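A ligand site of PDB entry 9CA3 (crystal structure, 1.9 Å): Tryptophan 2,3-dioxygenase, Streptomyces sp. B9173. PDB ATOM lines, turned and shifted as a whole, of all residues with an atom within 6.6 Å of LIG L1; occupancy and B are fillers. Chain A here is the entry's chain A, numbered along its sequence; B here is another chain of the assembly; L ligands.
The backbone NH of Leu 234 lies within hydrogen-bond range of an oxygen (O1) of LIG L1 (2.6 Å). A nitrogen (N1) of LIG L1 is in hydrogen-bond range of the backbone carbonyl oxygen (O) of Ala 127 (2.6 Å). NE of Arg 120 lies within salt-bridge range of O2 of LIG L1 (2.8 Å). NE2 of His 57 is in hydrogen-bond range of N2 of LIG L1, 3.2 Å away. A nitrogen (N1) of LG2 L2 is in hydrogen-bond range of the backbone NH (N) of Gly 129, at 3.0 Å. The side-chain hydroxyl (OG) of Ser 233 sits at hydrogen-bond distance from an oxygen (O4) of LG3 L3, at 2.8 Å.
A nitrogen (N1) of LIG L1 is in hydrogen-bond range of a nitrogen (N1) of LG2 L2 (2.8 Å).
O of Gln 232 sits at hydrogen-bond distance from NH2 of Arg 120 (2.4 Å). O of Phe 53 lies within hydrogen-bond range of ND1 of His 57. OG of Ser 233 lies close to N of Gly 235, at 3.0 Å.
Residues that only touch LIG L1: Phe 53, Leu 123, Thr 128, Leu 211, Ser 233, Tyr 26 of chain B and Val 29 of chain B. Hydrophobic or aromatic side chains within 4 Å of LIG L1: Phe 53, His 57, Leu 123, Ala 127, Leu 211, Leu 234, Tyr 26 of chain B and Val 29 of chain B. 11 residues have an atom within 4 Å of LIG L1: Phe 53, His 57, Arg 120, Leu 123, Ala 127, Thr 128, Leu 211, Ser 233, Leu 234, Tyr 26 of chain B and Val 29 of chain B.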
ATOM      1  N   PHE A  53      10.456 -28.512  28.401  1.00  0.00           N
ATOM      2  CA  PHE A  53       9.380 -27.833  27.697  1.00  0.00           C
ATOM      3  C   PHE A  53       9.208 -28.395  26.296  1.00  0.00           C
ATOM      4  O   PHE A  53       8.126 -28.882  25.923  1.00  0.00           O
ATOM      5  CB  PHE A  53       9.689 -26.326  27.679  1.00  0.00           C
ATOM      6  CG  PHE A  53       8.596 -25.449  27.115  1.00  0.00           C
ATOM      7  CD1 PHE A  53       8.581 -25.118  25.771  1.00  0.00           C
ATOM      8  CD2 PHE A  53       7.640 -24.891  27.939  1.00  0.00           C
ATOM      9  CE1 PHE A  53       7.602 -24.293  25.253  1.00  0.00           C
ATOM     10  CE2 PHE A  53       6.654 -24.070  27.427  1.00  0.00           C
ATOM     11  CZ  PHE A  53       6.643 -23.772  26.085  1.00  0.00           C
ATOM     12  N   HIS A  57       6.161 -31.234  24.225  1.00  0.00           N
ATOM     13  CA  HIS A  57       5.396 -30.847  23.046  1.00  0.00           C
ATOM     14  C   HIS A  57       5.638 -31.816  21.911  1.00  0.00           C
ATOM     15  O   HIS A  57       4.704 -32.227  21.206  1.00  0.00           O
ATOM     16  CB  HIS A  57       5.774 -29.436  22.592  1.00  0.00           C
ATOM     17  CG  HIS A  57       5.206 -28.343  23.427  1.00  0.00           C
ATOM     18  ND1 HIS A  57       5.803 -27.898  24.592  1.00  0.00           N
ATOM     19  CD2 HIS A  57       4.107 -27.576  23.252  1.00  0.00           C
ATOM     20  CE1 HIS A  57       5.084 -26.908  25.096  1.00  0.00           C
ATOM     21  NE2 HIS A  57       4.049 -26.691  24.301  1.00  0.00           N
ATOM     22  N   LEU A 116       8.735 -21.177  33.799  1.00  0.00           N
ATOM     23  CA  LEU A 116       7.872 -20.931  32.656  1.00  0.00           C
ATOM     24  C   LEU A 116       7.754 -19.443  32.387  1.00  0.00           C
ATOM     25  O   LEU A 116       7.840 -18.999  31.231  1.00  0.00           O
ATOM     26  CB  LEU A 116       6.498 -21.559  32.913  1.00  0.00           C
ATOM     27  CG  LEU A 116       5.389 -21.471  31.857  1.00  0.00           C
ATOM     28  CD1 LEU A 116       4.578 -20.184  32.065  1.00  0.00           C
ATOM     29  CD2 LEU A 116       5.936 -21.551  30.464  1.00  0.00           C
ATOM     30  N   ARG A 120       8.865 -17.573  29.072  1.00  0.00           N
ATOM     31  CA  ARG A 120       7.780 -16.939  28.333  1.00  0.00           C
ATOM     32  C   ARG A 120       8.067 -15.482  28.043  1.00  0.00           C
ATOM     33  O   ARG A 120       7.619 -14.956  27.017  1.00  0.00           O
ATOM     34  CB  ARG A 120       6.478 -17.070  29.137  1.00  0.00           C
ATOM     35  CG  ARG A 120       5.224 -16.710  28.407  1.00  0.00           C
ATOM     36  CD  ARG A 120       4.037 -16.907  29.330  1.00  0.00           C
ATOM     37  NE  ARG A 120       2.775 -16.577  28.685  1.00  0.00           N
ATOM     38  CZ  ARG A 120       2.136 -15.434  28.873  1.00  0.00           C
ATOM     39  NH1 ARG A 120       2.595 -14.511  29.699  1.00  0.00           N
ATOM     40  NH2 ARG A 120       0.999 -15.216  28.222  1.00  0.00           N
ATOM     41  N   LEU A 123       9.798 -15.486  24.788  1.00  0.00           N
ATOM     42  CA  LEU A 123       9.221 -16.190  23.658  1.00  0.00           C
ATOM     43  C   LEU A 123       8.649 -15.179  22.660  1.00  0.00           C
ATOM     44  O   LEU A 123       8.365 -14.038  23.025  1.00  0.00           O
ATOM     45  CB  LEU A 123       8.123 -17.137  24.145  1.00  0.00           C
ATOM     46  CG  LEU A 123       8.613 -18.457  24.722  1.00  0.00           C
ATOM     47  CD1 LEU A 123       7.421 -19.236  25.218  1.00  0.00           C
ATOM     48  CD2 LEU A 123       9.386 -19.243  23.682  1.00  0.00           C
ATOM     49  N   PRO A 124       8.470 -15.586  21.402  1.00  0.00           N
ATOM     50  CA  PRO A 124       7.862 -14.667  20.424  1.00  0.00           C
ATOM     51  C   PRO A 124       6.412 -14.357  20.747  1.00  0.00           C
ATOM     52  O   PRO A 124       5.759 -15.040  21.549  1.00  0.00           O
ATOM     53  CB  PRO A 124       7.979 -15.441  19.106  1.00  0.00           C
ATOM     54  CG  PRO A 124       9.100 -16.392  19.328  1.00  0.00           C
ATOM     55  CD  PRO A 124       8.941 -16.823  20.759  1.00  0.00           C
ATOM     56  N   ASP A 126       2.419 -14.126  19.787  1.00  0.00           N
ATOM     57  CA  ASP A 126       1.510 -15.096  19.158  1.00  0.00           C
ATOM     58  C   ASP A 126       2.220 -16.416  18.916  1.00  0.00           C
ATOM     59  O   ASP A 126       2.185 -16.995  17.827  1.00  0.00           O
ATOM     60  CB  ASP A 126       0.895 -14.543  17.872  1.00  0.00           C
ATOM     61  CG  ASP A 126      -0.409 -15.245  17.485  1.00  0.00           C
ATOM     62  OD1 ASP A 126      -1.229 -15.571  18.371  1.00  0.00           O
ATOM     63  OD2 ASP A 126      -0.612 -15.494  16.274  1.00  0.00           O
ATOM     64  N   ALA A 127       2.901 -16.899  19.951  1.00  0.00           N
ATOM     65  CA  ALA A 127       3.467 -18.240  19.982  1.00  0.00           C
ATOM     66  C   ALA A 127       2.461 -19.093  20.749  1.00  0.00           C
ATOM     67  O   ALA A 127       2.452 -19.095  21.984  1.00  0.00           O
ATOM     68  CB  ALA A 127       4.838 -18.235  20.650  1.00  0.00           C
ATOM     69  N   THR A 128       1.615 -19.799  20.004  1.00  0.00           N
ATOM     70  CA  THR A 128       0.385 -20.396  20.530  1.00  0.00           C
ATOM     71  C   THR A 128       0.159 -21.764  19.910  1.00  0.00           C
ATOM     72  O   THR A 128       0.460 -21.998  18.732  1.00  0.00           O
ATOM     73  CB  THR A 128      -0.855 -19.532  20.224  1.00  0.00           C
ATOM     74  OG1 THR A 128      -2.028 -20.297  20.464  1.00  0.00           O
ATOM     75  CG2 THR A 128      -0.887 -19.074  18.744  1.00  0.00           C
ATOM     76  N   GLY A 129      -0.441 -22.667  20.692  1.00  0.00           N
ATOM     77  CA  GLY A 129      -0.853 -23.982  20.202  1.00  0.00           C
ATOM     78  C   GLY A 129      -2.080 -23.973  19.304  1.00  0.00           C
ATOM     79  O   GLY A 129      -2.441 -25.033  18.775  1.00  0.00           O
ATOM     80  N   LEU A 211      -0.145 -19.575  34.439  1.00  0.00           N
ATOM     81  CA  LEU A 211      -0.495 -18.191  34.128  1.00  0.00           C
ATOM     82  C   LEU A 211      -1.513 -17.598  35.079  1.00  0.00           C
ATOM     83  O   LEU A 211      -1.692 -16.375  35.084  1.00  0.00           O
ATOM     84  CB  LEU A 211      -1.019 -18.089  32.688  1.00  0.00           C
ATOM     85  CG  LEU A 211      -0.057 -18.502  31.572  1.00  0.00           C
ATOM     86  CD1 LEU A 211      -0.641 -18.129  30.220  1.00  0.00           C
ATOM     87  CD2 LEU A 211       1.314 -17.867  31.757  1.00  0.00           C
ATOM     88  N   GLN A 232      -3.297 -13.163  29.962  1.00  0.00           N
ATOM     89  CA  GLN A 232      -3.420 -13.247  28.519  1.00  0.00           C
ATOM     90  C   GLN A 232      -2.372 -14.169  27.936  1.00  0.00           C
ATOM     91  O   GLN A 232      -1.243 -14.257  28.431  1.00  0.00           O
ATOM     92  CB  GLN A 232      -3.284 -11.873  27.862  1.00  0.00           C
ATOM     93  CG  GLN A 232      -4.103 -10.795  28.527  1.00  0.00           C
ATOM     94  CD  GLN A 232      -3.888  -9.428  27.887  1.00  0.00           C
ATOM     95  OE1 GLN A 232      -2.940  -9.231  27.132  1.00  0.00           O
ATOM     96  NE2 GLN A 232      -4.771  -8.481  28.221  1.00  0.00           N
ATOM     97  N   SER A 233      -2.756 -14.851  26.853  1.00  0.00           N
ATOM     98  CA  SER A 233      -1.847 -15.658  26.075  1.00  0.00           C
ATOM     99  C   SER A 233      -0.744 -14.797  25.450  1.00  0.00           C
ATOM    100  O   SER A 233      -0.747 -13.572  25.536  1.00  0.00           O
ATOM    101  CB  SER A 233      -2.622 -16.400  24.977  1.00  0.00           C
ATOM    102  OG  SER A 233      -2.827 -15.579  23.844  1.00  0.00           O
ATOM    103  N   LEU A 234       0.220 -15.467  24.824  1.00  0.00           N
ATOM    104  CA  LEU A 234       1.287 -14.814  24.059  1.00  0.00           C
ATOM    105  C   LEU A 234       0.768 -14.156  22.747  1.00  0.00           C
ATOM    106  O   LEU A 234       1.577 -13.672  21.939  1.00  0.00           O
ATOM    107  CB  LEU A 234       2.395 -15.820  23.731  1.00  0.00           C
ATOM    108  CG  LEU A 234       3.327 -16.162  24.894  1.00  0.00           C
ATOM    109  CD1 LEU A 234       4.496 -17.016  24.418  1.00  0.00           C
ATOM    110  CD2 LEU A 234       3.822 -14.890  25.562  1.00  0.00           C
ATOM    111  N   GLY A 235      -0.549 -14.172  22.559  1.00  0.00           N
ATOM    112  CA  GLY A 235      -1.206 -13.530  21.435  1.00  0.00           C
ATOM    113  C   GLY A 235      -2.173 -12.464  21.902  1.00  0.00           C
ATOM    114  O   GLY A 235      -2.939 -11.908  21.117  1.00  0.00           O
ATOM    115  N   ASN B  25       5.104 -19.305  14.879  1.00  0.00           N
ATOM    116  CA  ASN B  25       6.093 -19.183  15.939  1.00  0.00           C
ATOM    117  C   ASN B  25       6.052 -20.363  16.888  1.00  0.00           C
ATOM    118  O   ASN B  25       7.082 -20.797  17.411  1.00  0.00           O
ATOM    119  CB  ASN B  25       5.882 -17.872  16.700  1.00  0.00           C
ATOM    120  CG  ASN B  25       6.692 -16.726  16.123  1.00  0.00           C
ATOM    121  OD1 ASN B  25       7.756 -16.945  15.543  1.00  0.00           O
ATOM    122  ND2 ASN B  25       6.191 -15.500  16.269  1.00  0.00           N
ATOM    123  N   TYR B  26       4.856 -20.901  17.152  1.00  0.00           N
ATOM    124  CA  TYR B  26       4.762 -22.157  17.875  1.00  0.00           C
ATOM    125  C   TYR B  26       5.556 -23.243  17.178  1.00  0.00           C
ATOM    126  O   TYR B  26       6.319 -23.988  17.806  1.00  0.00           O
ATOM    127  CB  TYR B  26       3.294 -22.564  17.996  1.00  0.00           C
ATOM    128  CG  TYR B  26       3.038 -23.957  18.545  1.00  0.00           C
ATOM    129  CD1 TYR B  26       3.045 -25.073  17.705  1.00  0.00           C
ATOM    130  CD2 TYR B  26       2.754 -24.144  19.899  1.00  0.00           C
ATOM    131  CE1 TYR B  26       2.801 -26.346  18.208  1.00  0.00           C
ATOM    132  CE2 TYR B  26       2.509 -25.403  20.409  1.00  0.00           C
ATOM    133  CZ  TYR B  26       2.542 -26.505  19.557  1.00  0.00           C
ATOM    134  OH  TYR B  26       2.297 -27.752  20.073  1.00  0.00           O
ATOM    135  N   GLU B  27       5.386 -23.365  15.852  1.00  0.00           N
ATOM    136  CA  GLU B  27       6.156 -24.354  15.105  1.00  0.00           C
ATOM    137  C   GLU B  27       7.645 -24.051  15.184  1.00  0.00           C
ATOM    138  O   GLU B  27       8.471 -24.970  15.356  1.00  0.00           O
ATOM    139  CB  GLU B  27       5.691 -24.406  13.657  1.00  0.00           C
ATOM    140  CG  GLU B  27       4.532 -25.368  13.407  1.00  0.00           C
ATOM    141  CD  GLU B  27       3.720 -25.005  12.180  1.00  0.00           C
ATOM    142  OE1 GLU B  27       3.236 -23.857  12.096  1.00  0.00           O
ATOM    143  OE2 GLU B  27       3.518 -25.887  11.323  1.00  0.00           O
ATOM    144  N   VAL B  29       9.458 -22.387  17.481  1.00  0.00           N
ATOM    145  CA  VAL B  29      10.058 -22.599  18.801  1.00  0.00           C
ATOM    146  C   VAL B  29      10.408 -24.068  19.001  1.00  0.00           C
ATOM    147  O   VAL B  29      11.481 -24.389  19.541  1.00  0.00           O
ATOM    148  CB  VAL B  29       9.108 -22.085  19.907  1.00  0.00           C
ATOM    149  CG1 VAL B  29       9.617 -22.503  21.280  1.00  0.00           C
ATOM    150  CG2 VAL B  29       8.973 -20.580  19.849  1.00  0.00           C
ATOM    151  N   LEU B  30       9.542 -24.976  18.547  1.00  0.00           N
ATOM    152  CA  LEU B  30       9.687 -26.395  18.852  1.00  0.00           C
ATOM    153  C   LEU B  30      10.536 -27.175  17.850  1.00  0.00           C
ATOM    154  O   LEU B  30      10.753 -28.380  18.071  1.00  0.00           O
ATOM    155  CB  LEU B  30       8.305 -27.049  18.945  1.00  0.00           C
ATOM    156  CG  LEU B  30       7.454 -26.469  20.069  1.00  0.00           C
ATOM    157  CD1 LEU B  30       6.001 -26.904  19.907  1.00  0.00           C
ATOM    158  CD2 LEU B  30       8.024 -26.899  21.422  1.00  0.00           C
HETATM  159  O1  LIG L   1       0.518 -18.032  25.204  1.00  0.00           O
HETATM  160  C1  LIG L   1       1.177 -18.763  25.995  1.00  0.00           C
HETATM  161  O2  LIG L   1       1.340 -18.423  27.183  1.00  0.00           O
HETATM  162  C2  LIG L   1       1.741 -20.102  25.491  1.00  0.00           C
HETATM  163  N1  LIG L   1       1.377 -20.226  24.095  1.00  0.00           N
HETATM  164  C3  LIG L   1       3.255 -20.165  25.659  1.00  0.00           C
HETATM  165  C4  LIG L   1       3.653 -20.440  27.118  1.00  0.00           C
HETATM  166  C5  LIG L   1       3.809 -21.276  24.752  1.00  0.00           C
HETATM  167  C6  LIG L   1       4.520 -21.700  23.674  1.00  0.00           C
HETATM  168  C7  LIG L   1       5.240 -20.985  22.694  1.00  0.00           C
HETATM  169  C8  LIG L   1       5.888 -21.678  21.697  1.00  0.00           C
HETATM  170  C9  LIG L   1       5.831 -23.067  21.659  1.00  0.00           C
HETATM  171  C10 LIG L   1       5.124 -23.762  22.632  1.00  0.00           C
HETATM  172  C11 LIG L   1       4.449 -23.064  23.618  1.00  0.00           C
HETATM  173  N2  LIG L   1       3.703 -23.497  24.697  1.00  0.00           N
HETATM  174  C12 LIG L   1       3.307 -22.397  25.392  1.00  0.00           C
HETATM  175  C1  LG2 L   2       0.378 -23.928  23.820  1.00  0.00           C
HETATM  176  N1  LG2 L   2       0.516 -22.822  23.567  1.00  0.00           N
HETATM  177  C1  LG3 L   3      -3.621 -23.097  23.664  1.00  0.00           C
HETATM  178  C2  LG3 L   3      -1.255 -27.300  23.123  1.00  0.00           C
HETATM  179  C3  LG3 L   3       1.511 -26.155  26.966  1.00  0.00           C
HETATM  180  C4  LG3 L   3      -0.861 -21.993  27.494  1.00  0.00           C
HETATM  181  C5  LG3 L   3      -3.263 -24.355  23.235  1.00  0.00           C
HETATM  182  C6  LG3 L   3      -3.972 -25.125  22.240  1.00  0.00           C
HETATM  183  C7  LG3 L   3      -3.316 -26.276  22.098  1.00  0.00           C
HETATM  184  C8  LG3 L   3      -2.174 -26.281  22.984  1.00  0.00           C
HETATM  185  C9  LG3 L   3      -3.672 -27.444  21.167  1.00  0.00           C
HETATM  186  C10 LG3 L   3      -5.265 -24.669  21.522  1.00  0.00           C
HETATM  187  C11 LG3 L   3      -6.426 -25.408  22.184  1.00  0.00           C
HETATM  188  C12 LG3 L   3      -7.759 -24.684  22.079  1.00  0.00           C
HETATM  189  O1  LG3 L   3      -8.797 -25.300  22.439  1.00  0.00           O
HETATM  190  O2  LG3 L   3      -7.791 -23.495  21.655  1.00  0.00           O
HETATM  191  C13 LG3 L   3      -0.307 -27.353  24.135  1.00  0.00           C
HETATM  192  C14 LG3 L   3       0.590 -28.452  24.409  1.00  0.00           C
HETATM  193  C15 LG3 L   3       1.341 -28.111  25.478  1.00  0.00           C
HETATM  194  C16 LG3 L   3       0.927 -26.806  25.904  1.00  0.00           C
HETATM  195  C17 LG3 L   3       0.626 -29.742  23.566  1.00  0.00           C
HETATM  196  C18 LG3 L   3       2.460 -28.889  26.221  1.00  0.00           C
HETATM  197  C19 LG3 L   3       2.693 -30.193  26.055  1.00  0.00           C
HETATM  198  C20 LG3 L   3       1.164 -24.909  27.433  1.00  0.00           C
HETATM  199  C21 LG3 L   3       1.809 -24.170  28.499  1.00  0.00           C
HETATM  200  C22 LG3 L   3       1.121 -23.018  28.623  1.00  0.00           C
HETATM  201  C23 LG3 L   3       0.054 -23.010  27.661  1.00  0.00           C
HETATM  202  C24 LG3 L   3       3.049 -24.661  29.297  1.00  0.00           C
HETATM  203  C25 LG3 L   3       1.318 -21.817  29.573  1.00  0.00           C
HETATM  204  C26 LG3 L   3       2.119 -21.875  30.629  1.00  0.00           C
HETATM  205  C27 LG3 L   3      -1.807 -21.927  26.475  1.00  0.00           C
HETATM  206  C28 LG3 L   3      -2.702 -20.811  26.228  1.00  0.00           C
HETATM  207  C29 LG3 L   3      -3.465 -21.098  25.177  1.00  0.00           C
HETATM  208  C30 LG3 L   3      -3.077 -22.423  24.727  1.00  0.00           C
HETATM  209  C31 LG3 L   3      -2.714 -19.519  27.068  1.00  0.00           C
HETATM  210  C32 LG3 L   3      -4.554 -20.216  24.542  1.00  0.00           C
HETATM  211  C33 LG3 L   3      -3.984 -19.598  23.267  1.00  0.00           C
HETATM  212  C34 LG3 L   3      -4.816 -18.405  22.847  1.00  0.00           C
HETATM  213  O3  LG3 L   3      -6.056 -18.427  23.070  1.00  0.00           O
HETATM  214  O4  LG3 L   3      -4.242 -17.444  22.273  1.00  0.00           O
HETATM  215  N1  LG3 L   3      -2.168 -25.081  23.665  1.00  0.00           N
HETATM  216  N2  LG3 L   3      -0.076 -26.372  25.063  1.00  0.00           N
HETATM  217  N3  LG3 L   3       0.101 -24.182  26.943  1.00  0.00           N
HETATM  218  N4  LG3 L   3      -2.067 -22.892  25.542  1.00  0.00           N
HETATM  219 FE1  LG3 L   3      -1.034 -24.559  25.265  1.00  0.00          FE
